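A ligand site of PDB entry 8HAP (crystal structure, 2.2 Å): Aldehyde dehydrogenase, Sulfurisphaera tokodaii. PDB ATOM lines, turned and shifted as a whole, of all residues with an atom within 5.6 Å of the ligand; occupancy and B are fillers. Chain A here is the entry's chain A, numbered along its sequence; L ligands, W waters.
The backbone carbonyl oxygen of Leu 150 is in hydrogen-bond range of an oxygen (O5) of the ligand (2.6 Å).
OE1 of Glu 381 sits at hydrogen-bond distance from O12 of the ligand (2.7 Å).
An oxygen (O14) of the ligand sits at hydrogen-bond distance from the side-chain hydroxyl (OG) of Ser 209.
An oxygen (O16) of the ligand is in salt-bridge range of the side-chain amino group of Lys 176, 3.5 Å away.
N of Ser 230 is in hydrogen-bond range of O1 of the ligand (2.9 Å).
The side-chain hydroxyl (OG) of Ser 230 lies within hydrogen-bond range of an oxygen (O1) of the ligand, 2.9 Å away.
An oxygen (O16) of the ligand lies within hydrogen-bond range of the backbone NH of Ile 179, 2.9 Å away.
O13 of the ligand lies within hydrogen-bond range of O of Gly 229 (3.0 Å).
O of Leu 252 is in hydrogen-bond range of O13 of the ligand.
The side-chain hydroxyl of Ser 178 sits at hydrogen-bond distance from an oxygen (O15) of the ligand, 3.1 Å away.
The backbone NH of Phe 152 sits at hydrogen-bond distance from an oxygen (O9) of the ligand (3.2 Å).
N of Leu 150 is in hydrogen-bond range of O of Lys 176 (3.1 Å).
The backbone NH (N) of Gly 254 lies within hydrogen-bond range of the side-chain carboxylate (OE2) of Glu 381 (3.0 Å).
The side-chain hydroxyl (OG) of Ser 230 is in hydrogen-bond range of the side-chain hydroxyl (OG1) of Thr 233 (3.1 Å).
The backbone carbonyl oxygen (O) of Glu 251 sits at hydrogen-bond distance from the backbone NH (N) of Gly 229 (3.2 Å).
OG of Ser 178 sits close to N of Ser 180.
N of Thr 228 sits at hydrogen-bond distance from O of Ile 149, at 3.3 Å.
The backbone carbonyl oxygen (O) of Leu 227 is in hydrogen-bond range of the backbone NH (N) of Glu 251 (2.9 Å).
Merely in contact with the ligand: Ile 149 (3.1 Å), Thr 233 (3.2 Å), Cys 285 (3.4 Å), Gly 213 (3.4 Å), Pro 151 (3.4 Å), Glu 251 (3.5 Å), Ile 237 (3.6 Å), Thr 228 (3.6 Å), Gly 253 (3.6 Å), Phe 383 (3.6 Å), Asn 153 (3.7 Å) and Pro 177 (3.9 Å).
Hydrophobic or aromatic side chains that line the ligand: Ile 149, Pro 151, Phe 152, Ile 179, Ile 237 and Phe 383.
Of the 31 residues printed, 22 come within 4 Å of the ligand.
Water W3 lies within hydrogen-bond range of N4 of the ligand and OD1 of Asp 214.
Water W2 bridges the side-chain hydroxyl (OG) of Ser 209 and an oxygen (O14) of the ligand.
Water W1 bridges SG of Cys 285 and ND2 of Asn 153.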
ATOM      1  N   ILE A 149     -25.060 -10.074 -18.091  1.00  0.00           N
ATOM      2  CA  ILE A 149     -24.826 -10.216 -19.557  1.00  0.00           C
ATOM      3  C   ILE A 149     -24.146  -8.951 -20.061  1.00  0.00           C
ATOM      4  O   ILE A 149     -24.780  -7.929 -20.033  1.00  0.00           O
ATOM      5  CB  ILE A 149     -26.156 -10.507 -20.254  1.00  0.00           C
ATOM      6  CG1 ILE A 149     -26.633 -11.899 -19.830  1.00  0.00           C
ATOM      7  CG2 ILE A 149     -25.970 -10.390 -21.750  1.00  0.00           C
ATOM      8  CD1 ILE A 149     -28.033 -12.238 -20.215  1.00  0.00           C
ATOM      9  N   LEU A 150     -22.870  -9.041 -20.411  1.00  0.00           N
ATOM     10  CA  LEU A 150     -22.033  -7.854 -20.672  1.00  0.00           C
ATOM     11  C   LEU A 150     -22.060  -7.505 -22.145  1.00  0.00           C
ATOM     12  O   LEU A 150     -22.184  -8.374 -23.002  1.00  0.00           O
ATOM     13  CB  LEU A 150     -20.591  -8.102 -20.220  1.00  0.00           C
ATOM     14  CG  LEU A 150     -20.472  -8.655 -18.804  1.00  0.00           C
ATOM     15  CD1 LEU A 150     -19.029  -8.661 -18.354  1.00  0.00           C
ATOM     16  CD2 LEU A 150     -21.342  -7.838 -17.880  1.00  0.00           C
ATOM     17  N   PRO A 151     -21.906  -6.187 -22.442  1.00  0.00           N
ATOM     18  CA  PRO A 151     -21.713  -5.704 -23.797  1.00  0.00           C
ATOM     19  C   PRO A 151     -20.246  -5.906 -24.196  1.00  0.00           C
ATOM     20  O   PRO A 151     -19.383  -6.127 -23.338  1.00  0.00           O
ATOM     21  CB  PRO A 151     -22.060  -4.212 -23.670  1.00  0.00           C
ATOM     22  CG  PRO A 151     -21.615  -3.830 -22.248  1.00  0.00           C
ATOM     23  CD  PRO A 151     -21.817  -5.102 -21.437  1.00  0.00           C
ATOM     24  N   PHE A 152     -19.956  -5.821 -25.492  1.00  0.00           N
ATOM     25  CA  PHE A 152     -18.592  -6.001 -26.025  1.00  0.00           C
ATOM     26  C   PHE A 152     -17.786  -4.731 -25.743  1.00  0.00           C
ATOM     27  O   PHE A 152     -16.568  -4.811 -25.661  1.00  0.00           O
ATOM     28  CB  PHE A 152     -18.634  -6.377 -27.498  1.00  0.00           C
ATOM     29  CG  PHE A 152     -18.975  -5.224 -28.399  1.00  0.00           C
ATOM     30  CD1 PHE A 152     -18.002  -4.334 -28.786  1.00  0.00           C
ATOM     31  CD2 PHE A 152     -20.267  -5.030 -28.867  1.00  0.00           C
ATOM     32  CE1 PHE A 152     -18.303  -3.248 -29.583  1.00  0.00           C
ATOM     33  CE2 PHE A 152     -20.562  -3.956 -29.661  1.00  0.00           C
ATOM     34  CZ  PHE A 152     -19.573  -3.062 -30.021  1.00  0.00           C
ATOM     35  N   ASN A 153     -18.441  -3.565 -25.602  1.00  0.00           N
ATOM     36  CA  ASN A 153     -17.776  -2.254 -25.789  1.00  0.00           C
ATOM     37  C   ASN A 153     -17.160  -1.721 -24.475  1.00  0.00           C
ATOM     38  O   ASN A 153     -16.267  -0.845 -24.557  1.00  0.00           O
ATOM     39  CB  ASN A 153     -18.719  -1.247 -26.423  1.00  0.00           C
ATOM     40  CG  ASN A 153     -19.874  -0.825 -25.534  1.00  0.00           C
ATOM     41  OD1 ASN A 153     -20.377  -1.622 -24.750  1.00  0.00           O
ATOM     42  ND2 ASN A 153     -20.279   0.428 -25.647  1.00  0.00           N
ATOM     43  N   LYS A 176     -21.840 -13.560 -18.094  1.00  0.00           N
ATOM     44  CA  LYS A 176     -21.651 -13.961 -19.522  1.00  0.00           C
ATOM     45  C   LYS A 176     -21.127 -12.755 -20.285  1.00  0.00           C
ATOM     46  O   LYS A 176     -21.900 -11.921 -20.748  1.00  0.00           O
ATOM     47  CB  LYS A 176     -22.940 -14.443 -20.186  1.00  0.00           C
ATOM     48  CG  LYS A 176     -22.692 -15.152 -21.521  1.00  0.00           C
ATOM     49  CD  LYS A 176     -23.902 -15.192 -22.438  1.00  0.00           C
ATOM     50  CE  LYS A 176     -24.097 -13.889 -23.178  1.00  0.00           C
ATOM     51  NZ  LYS A 176     -22.884 -13.522 -23.967  1.00  0.00           N
ATOM     52  N   PRO A 177     -19.811 -12.679 -20.530  1.00  0.00           N
ATOM     53  CA  PRO A 177     -19.274 -11.598 -21.356  1.00  0.00           C
ATOM     54  C   PRO A 177     -19.717 -11.853 -22.792  1.00  0.00           C
ATOM     55  O   PRO A 177     -20.184 -12.939 -23.119  1.00  0.00           O
ATOM     56  CB  PRO A 177     -17.766 -11.699 -21.190  1.00  0.00           C
ATOM     57  CG  PRO A 177     -17.546 -13.176 -20.841  1.00  0.00           C
ATOM     58  CD  PRO A 177     -18.784 -13.627 -20.098  1.00  0.00           C
ATOM     59  N   SER A 178     -19.650 -10.804 -23.610  1.00  0.00           N
ATOM     60  CA  SER A 178     -19.819 -10.939 -25.081  1.00  0.00           C
ATOM     61  C   SER A 178     -18.767 -11.932 -25.603  1.00  0.00           C
ATOM     62  O   SER A 178     -17.620 -11.909 -25.123  1.00  0.00           O
ATOM     63  CB  SER A 178     -19.717  -9.582 -25.705  1.00  0.00           C
ATOM     64  OG  SER A 178     -19.567  -9.684 -27.102  1.00  0.00           O
ATOM     65  N   ILE A 179     -19.147 -12.815 -26.520  1.00  0.00           N
ATOM     66  CA  ILE A 179     -18.212 -13.768 -27.167  1.00  0.00           C
ATOM     67  C   ILE A 179     -17.209 -12.989 -28.016  1.00  0.00           C
ATOM     68  O   ILE A 179     -16.125 -13.525 -28.268  1.00  0.00           O
ATOM     69  CB  ILE A 179     -18.959 -14.840 -27.980  1.00  0.00           C
ATOM     70  CG1 ILE A 179     -18.012 -16.001 -28.318  1.00  0.00           C
ATOM     71  CG2 ILE A 179     -19.598 -14.239 -29.230  1.00  0.00           C
ATOM     72  CD1 ILE A 179     -17.262 -16.551 -27.105  1.00  0.00           C
ATOM     73  N   SER A 180     -17.513 -11.737 -28.392  1.00  0.00           N
ATOM     74  CA  SER A 180     -16.533 -10.814 -29.032  1.00  0.00           C
ATOM     75  C   SER A 180     -15.393 -10.446 -28.064  1.00  0.00           C
ATOM     76  O   SER A 180     -14.278 -10.202 -28.557  1.00  0.00           O
ATOM     77  CB  SER A 180     -17.202  -9.587 -29.539  1.00  0.00           C
ATOM     78  OG  SER A 180     -18.230  -9.928 -30.453  1.00  0.00           O
ATOM     79  N   GLY A 207     -19.575 -18.870 -24.493  1.00  0.00           N
ATOM     80  CA  GLY A 207     -20.360 -19.685 -25.431  1.00  0.00           C
ATOM     81  C   GLY A 207     -21.158 -18.815 -26.364  1.00  0.00           C
ATOM     82  O   GLY A 207     -21.078 -17.581 -26.263  1.00  0.00           O
ATOM     83  N   SER A 209     -24.695 -17.364 -27.715  1.00  0.00           N
ATOM     84  CA  SER A 209     -25.983 -16.937 -27.096  1.00  0.00           C
ATOM     85  C   SER A 209     -27.070 -17.981 -27.373  1.00  0.00           C
ATOM     86  O   SER A 209     -27.884 -18.224 -26.455  1.00  0.00           O
ATOM     87  CB  SER A 209     -26.400 -15.572 -27.607  1.00  0.00           C
ATOM     88  OG  SER A 209     -25.334 -14.646 -27.537  1.00  0.00           O
ATOM     89  N   GLY A 213     -27.627 -18.837 -23.815  1.00  0.00           N
ATOM     90  CA  GLY A 213     -28.449 -17.653 -23.487  1.00  0.00           C
ATOM     91  C   GLY A 213     -29.578 -18.011 -22.527  1.00  0.00           C
ATOM     92  O   GLY A 213     -29.637 -17.421 -21.430  1.00  0.00           O
ATOM     93  N   ASP A 214     -30.377 -19.028 -22.901  1.00  0.00           N
ATOM     94  CA  ASP A 214     -31.716 -19.300 -22.313  1.00  0.00           C
ATOM     95  C   ASP A 214     -31.599 -19.782 -20.853  1.00  0.00           C
ATOM     96  O   ASP A 214     -32.307 -19.232 -20.005  1.00  0.00           O
ATOM     97  CB  ASP A 214     -32.499 -20.278 -23.176  1.00  0.00           C
ATOM     98  CG  ASP A 214     -33.916 -19.803 -23.358  1.00  0.00           C
ATOM     99  OD1 ASP A 214     -34.067 -18.679 -23.867  1.00  0.00           O
ATOM    100  OD2 ASP A 214     -34.840 -20.513 -22.914  1.00  0.00           O
ATOM    101  N   ILE A 217     -31.253 -17.180 -18.191  1.00  0.00           N
ATOM    102  CA  ILE A 217     -32.468 -16.331 -18.020  1.00  0.00           C
ATOM    103  C   ILE A 217     -33.576 -17.124 -17.315  1.00  0.00           C
ATOM    104  O   ILE A 217     -34.428 -16.474 -16.666  1.00  0.00           O
ATOM    105  CB  ILE A 217     -32.954 -15.774 -19.384  1.00  0.00           C
ATOM    106  CG1 ILE A 217     -31.854 -14.998 -20.114  1.00  0.00           C
ATOM    107  CG2 ILE A 217     -34.183 -14.913 -19.191  1.00  0.00           C
ATOM    108  CD1 ILE A 217     -31.079 -14.014 -19.241  1.00  0.00           C
ATOM    109  N   LEU A 227     -28.375  -6.578 -17.691  1.00  0.00           N
ATOM    110  CA  LEU A 227     -27.927  -6.653 -19.081  1.00  0.00           C
ATOM    111  C   LEU A 227     -27.641  -5.252 -19.628  1.00  0.00           C
ATOM    112  O   LEU A 227     -28.522  -4.368 -19.554  1.00  0.00           O
ATOM    113  CB  LEU A 227     -29.044  -7.333 -19.874  1.00  0.00           C
ATOM    114  CG  LEU A 227     -28.773  -7.454 -21.374  1.00  0.00           C
ATOM    115  CD1 LEU A 227     -29.313  -8.775 -21.907  1.00  0.00           C
ATOM    116  CD2 LEU A 227     -29.368  -6.279 -22.124  1.00  0.00           C
ATOM    117  N   THR A 228     -26.452  -5.074 -20.212  1.00  0.00           N
ATOM    118  CA  THR A 228     -26.161  -3.940 -21.120  1.00  0.00           C
ATOM    119  C   THR A 228     -26.056  -4.551 -22.527  1.00  0.00           C
ATOM    120  O   THR A 228     -25.393  -5.581 -22.653  1.00  0.00           O
ATOM    121  CB  THR A 228     -24.931  -3.161 -20.610  1.00  0.00           C
ATOM    122  OG1 THR A 228     -25.092  -2.849 -19.226  1.00  0.00           O
ATOM    123  CG2 THR A 228     -24.697  -1.894 -21.405  1.00  0.00           C
ATOM    124  N   GLY A 229     -26.721  -3.970 -23.534  1.00  0.00           N
ATOM    125  CA  GLY A 229     -26.789  -4.504 -24.916  1.00  0.00           C
ATOM    126  C   GLY A 229     -27.753  -3.700 -25.776  1.00  0.00           C
ATOM    127  O   GLY A 229     -28.044  -2.533 -25.413  1.00  0.00           O
ATOM    128  N   SER A 230     -28.210  -4.261 -26.892  1.00  0.00           N
ATOM    129  CA  SER A 230     -29.150  -3.578 -27.829  1.00  0.00           C
ATOM    130  C   SER A 230     -30.568  -3.698 -27.288  1.00  0.00           C
ATOM    131  O   SER A 230     -30.814  -4.578 -26.406  1.00  0.00           O
ATOM    132  CB  SER A 230     -29.055  -4.128 -29.230  1.00  0.00           C
ATOM    133  OG  SER A 230     -29.460  -5.485 -29.252  1.00  0.00           O
ATOM    134  N   THR A 231     -31.455  -2.820 -27.761  1.00  0.00           N
ATOM    135  CA  THR A 231     -32.894  -2.745 -27.385  1.00  0.00           C
ATOM    136  C   THR A 231     -33.586  -4.045 -27.809  1.00  0.00           C
ATOM    137  O   THR A 231     -34.316  -4.627 -26.964  1.00  0.00           O
ATOM    138  CB  THR A 231     -33.553  -1.491 -27.997  1.00  0.00           C
ATOM    139  OG1 THR A 231     -33.201  -0.354 -27.206  1.00  0.00           O
ATOM    140  CG2 THR A 231     -35.057  -1.587 -28.057  1.00  0.00           C
ATOM    141  N   THR A 233     -32.530  -7.189 -28.451  1.00  0.00           N
ATOM    142  CA  THR A 233     -32.012  -8.351 -27.667  1.00  0.00           C
ATOM    143  C   THR A 233     -32.481  -8.235 -26.210  1.00  0.00           C
ATOM    144  O   THR A 233     -32.975  -9.235 -25.657  1.00  0.00           O
ATOM    145  CB  THR A 233     -30.482  -8.420 -27.810  1.00  0.00           C
ATOM    146  OG1 THR A 233     -30.187  -8.534 -29.201  1.00  0.00           O
ATOM    147  CG2 THR A 233     -29.862  -9.584 -27.067  1.00  0.00           C
ATOM    148  N   GLY A 234     -32.344  -7.042 -25.624  1.00  0.00           N
ATOM    149  CA  GLY A 234     -32.676  -6.737 -24.225  1.00  0.00           C
ATOM    150  C   GLY A 234     -34.144  -6.930 -23.918  1.00  0.00           C
ATOM    151  O   GLY A 234     -34.464  -7.630 -22.933  1.00  0.00           O
ATOM    152  N   ILE A 237     -35.194 -10.570 -23.798  1.00  0.00           N
ATOM    153  CA  ILE A 237     -34.637 -11.265 -22.612  1.00  0.00           C
ATOM    154  C   ILE A 237     -35.449 -10.818 -21.387  1.00  0.00           C
ATOM    155  O   ILE A 237     -35.888 -11.702 -20.602  1.00  0.00           O
ATOM    156  CB  ILE A 237     -33.130 -10.965 -22.502  1.00  0.00           C
ATOM    157  CG1 ILE A 237     -32.322 -11.900 -23.413  1.00  0.00           C
ATOM    158  CG2 ILE A 237     -32.648 -11.020 -21.063  1.00  0.00           C
ATOM    159  CD1 ILE A 237     -30.848 -11.546 -23.501  1.00  0.00           C
ATOM    160  N   GLU A 251     -29.731  -1.735 -19.428  1.00  0.00           N
ATOM    161  CA  GLU A 251     -29.072  -0.535 -20.016  1.00  0.00           C
ATOM    162  C   GLU A 251     -28.959  -0.795 -21.521  1.00  0.00           C
ATOM    163  O   GLU A 251     -28.055  -1.547 -21.931  1.00  0.00           O
ATOM    164  CB  GLU A 251     -27.723  -0.271 -19.347  1.00  0.00           C
ATOM    165  CG  GLU A 251     -27.819  -0.051 -17.846  1.00  0.00           C
ATOM    166  CD  GLU A 251     -28.467   1.268 -17.442  1.00  0.00           C
ATOM    167  OE1 GLU A 251     -27.801   2.310 -17.608  1.00  0.00           O
ATOM    168  OE2 GLU A 251     -29.643   1.247 -16.966  1.00  0.00           O
ATOM    169  N   LEU A 252     -29.889  -0.275 -22.310  1.00  0.00           N
ATOM    170  CA  LEU A 252     -29.989  -0.616 -23.738  1.00  0.00           C
ATOM    171  C   LEU A 252     -29.513   0.594 -24.567  1.00  0.00           C
ATOM    172  O   LEU A 252     -28.726   1.439 -24.027  1.00  0.00           O
ATOM    173  CB  LEU A 252     -31.432  -1.073 -24.019  1.00  0.00           C
ATOM    174  CG  LEU A 252     -31.996  -2.098 -23.022  1.00  0.00           C
ATOM    175  CD1 LEU A 252     -33.437  -2.461 -23.319  1.00  0.00           C
ATOM    176  CD2 LEU A 252     -31.142  -3.357 -22.988  1.00  0.00           C
ATOM    177  N   GLY A 253     -29.878   0.683 -25.827  1.00  0.00           N
ATOM    178  CA  GLY A 253     -29.271   1.662 -26.756  1.00  0.00           C
ATOM    179  C   GLY A 253     -29.505   3.138 -26.405  1.00  0.00           C
ATOM    180  O   GLY A 253     -30.356   3.468 -25.563  1.00  0.00           O
ATOM    181  N   GLY A 254     -28.742   3.999 -27.080  1.00  0.00           N
ATOM    182  CA  GLY A 254     -28.985   5.439 -27.203  1.00  0.00           C
ATOM    183  C   GLY A 254     -28.737   5.916 -28.619  1.00  0.00           C
ATOM    184  O   GLY A 254     -27.952   5.280 -29.354  1.00  0.00           O
ATOM    185  N   ASN A 284     -20.311   3.647 -28.465  1.00  0.00           N
ATOM    186  CA  ASN A 284     -20.691   4.037 -27.090  1.00  0.00           C
ATOM    187  C   ASN A 284     -22.199   4.217 -27.024  1.00  0.00           C
ATOM    188  O   ASN A 284     -22.731   4.863 -27.907  1.00  0.00           O
ATOM    189  CB  ASN A 284     -19.967   5.305 -26.664  1.00  0.00           C
ATOM    190  CG  ASN A 284     -18.500   5.037 -26.412  1.00  0.00           C
ATOM    191  OD1 ASN A 284     -18.153   4.283 -25.504  1.00  0.00           O
ATOM    192  ND2 ASN A 284     -17.623   5.656 -27.202  1.00  0.00           N
ATOM    193  N   CYS A 285     -22.842   3.646 -25.999  1.00  0.00           N
ATOM    194  CA  CYS A 285     -24.296   3.828 -25.713  1.00  0.00           C
ATOM    195  C   CYS A 285     -24.607   5.331 -25.681  1.00  0.00           C
ATOM    196  O   CYS A 285     -25.644   5.665 -26.239  1.00  0.00           O
ATOM    197  CB  CYS A 285     -24.729   3.139 -24.412  1.00  0.00           C
ATOM    198  SG  CYS A 285     -23.927   3.812 -22.931  1.00  0.00           S
ATOM    199  N   GLU A 381     -29.991   3.323 -33.688  1.00  0.00           N
ATOM    200  CA  GLU A 381     -28.670   3.477 -33.014  1.00  0.00           C
ATOM    201  C   GLU A 381     -27.576   3.125 -34.016  1.00  0.00           C
ATOM    202  O   GLU A 381     -27.488   1.934 -34.384  1.00  0.00           O
ATOM    203  CB  GLU A 381     -28.574   2.584 -31.776  1.00  0.00           C
ATOM    204  CG  GLU A 381     -27.219   2.652 -31.096  1.00  0.00           C
ATOM    205  CD  GLU A 381     -27.184   2.052 -29.703  1.00  0.00           C
ATOM    206  OE1 GLU A 381     -27.730   0.933 -29.551  1.00  0.00           O
ATOM    207  OE2 GLU A 381     -26.627   2.707 -28.770  1.00  0.00           O
ATOM    208  N   PHE A 383     -23.960   2.419 -34.173  1.00  0.00           N
ATOM    209  CA  PHE A 383     -22.826   1.974 -33.329  1.00  0.00           C
ATOM    210  C   PHE A 383     -21.579   1.872 -34.229  1.00  0.00           C
ATOM    211  O   PHE A 383     -21.049   0.792 -34.432  1.00  0.00           O
ATOM    212  CB  PHE A 383     -23.247   0.664 -32.643  1.00  0.00           C
ATOM    213  CG  PHE A 383     -22.899   0.616 -31.179  1.00  0.00           C
ATOM    214  CD1 PHE A 383     -23.501   1.508 -30.298  1.00  0.00           C
ATOM    215  CD2 PHE A 383     -21.964  -0.283 -30.689  1.00  0.00           C
ATOM    216  CE1 PHE A 383     -23.178   1.484 -28.952  1.00  0.00           C
ATOM    217  CE2 PHE A 383     -21.649  -0.301 -29.333  1.00  0.00           C
ATOM    218  CZ  PHE A 383     -22.255   0.586 -28.470  1.00  0.00           C
HETATM  219  P1  LIG L   1     -25.911  -7.083 -28.000  1.00  0.00           P
HETATM  220  O1  LIG L   1     -27.373  -6.918 -27.739  1.00  0.00           O
HETATM  221  O2  LIG L   1     -25.477  -7.499 -29.368  1.00  0.00           O
HETATM  222  O3  LIG L   1     -25.303  -8.108 -26.924  1.00  0.00           O
HETATM  223  C1  LIG L   1     -25.294  -7.777 -25.516  1.00  0.00           C
HETATM  224  C2  LIG L   1     -25.009  -9.046 -24.751  1.00  0.00           C
HETATM  225  O4  LIG L   1     -26.193  -9.883 -24.833  1.00  0.00           O
HETATM  226  C3  LIG L   1     -23.855  -9.900 -25.289  1.00  0.00           C
HETATM  227  O5  LIG L   1     -23.130 -10.484 -24.199  1.00  0.00           O
HETATM  228  C4  LIG L   1     -24.583 -10.942 -26.125  1.00  0.00           C
HETATM  229  O6  LIG L   1     -23.906 -12.189 -26.290  1.00  0.00           O
HETATM  230  C5  LIG L   1     -25.792 -11.176 -25.236  1.00  0.00           C
HETATM  231  N1  LIG L   1     -26.909 -11.841 -25.885  1.00  0.00           N
HETATM  232  C6  LIG L   1     -27.389 -11.650 -27.150  1.00  0.00           C
HETATM  233  N2  LIG L   1     -28.425 -12.404 -27.431  1.00  0.00           N
HETATM  234  C7  LIG L   1     -28.635 -13.145 -26.267  1.00  0.00           C
HETATM  235  C8  LIG L   1     -29.581 -14.125 -25.924  1.00  0.00           C
HETATM  236  N3  LIG L   1     -30.554 -14.517 -26.740  1.00  0.00           N
HETATM  237  N4  LIG L   1     -29.505 -14.657 -24.685  1.00  0.00           N
HETATM  238  C9  LIG L   1     -28.532 -14.239 -23.855  1.00  0.00           C
HETATM  239  N5  LIG L   1     -27.596 -13.324 -24.073  1.00  0.00           N
HETATM  240  C10 LIG L   1     -27.701 -12.814 -25.310  1.00  0.00           C
HETATM  241  O7  LIG L   1     -25.134  -5.750 -27.593  1.00  0.00           O
HETATM  242  P2  LIG L   1     -23.604  -5.313 -27.841  1.00  0.00           P
HETATM  243  O8  LIG L   1     -23.436  -5.193 -29.313  1.00  0.00           O
HETATM  244  O9  LIG L   1     -22.722  -6.216 -27.022  1.00  0.00           O
HETATM  245  O10 LIG L   1     -23.545  -3.841 -27.221  1.00  0.00           O
HETATM  246  C11 LIG L   1     -24.319  -2.790 -27.827  1.00  0.00           C
HETATM  247  C12 LIG L   1     -24.909  -1.959 -26.721  1.00  0.00           C
HETATM  248  O11 LIG L   1     -23.892  -1.669 -25.738  1.00  0.00           O
HETATM  249  C13 LIG L   1     -25.487  -0.601 -27.113  1.00  0.00           C
HETATM  250  O12 LIG L   1     -26.769  -0.756 -27.720  1.00  0.00           O
HETATM  251  C14 LIG L   1     -25.385   0.123 -25.758  1.00  0.00           C
HETATM  252  O13 LIG L   1     -26.254  -0.279 -24.712  1.00  0.00           O
HETATM  253  C15 LIG L   1     -23.988  -0.303 -25.321  1.00  0.00           C
HETATM  254  P3  LIG L   1     -22.971 -12.198 -27.639  1.00  0.00           P
HETATM  255  O14 LIG L   1     -23.876 -12.578 -28.778  1.00  0.00           O
HETATM  256  O15 LIG L   1     -22.347 -10.821 -27.835  1.00  0.00           O
HETATM  257  O16 LIG L   1     -21.936 -13.249 -27.306  1.00  0.00           O
HETATM  258  O   HOH W   1     -22.083   2.050 -23.857  1.00  0.00           O
HETATM  259  O   HOH W   2     -23.353 -15.488 -29.302  1.00  0.00           O
HETATM  260  O   HOH W   3     -32.096 -15.916 -23.902  1.00  0.00           O
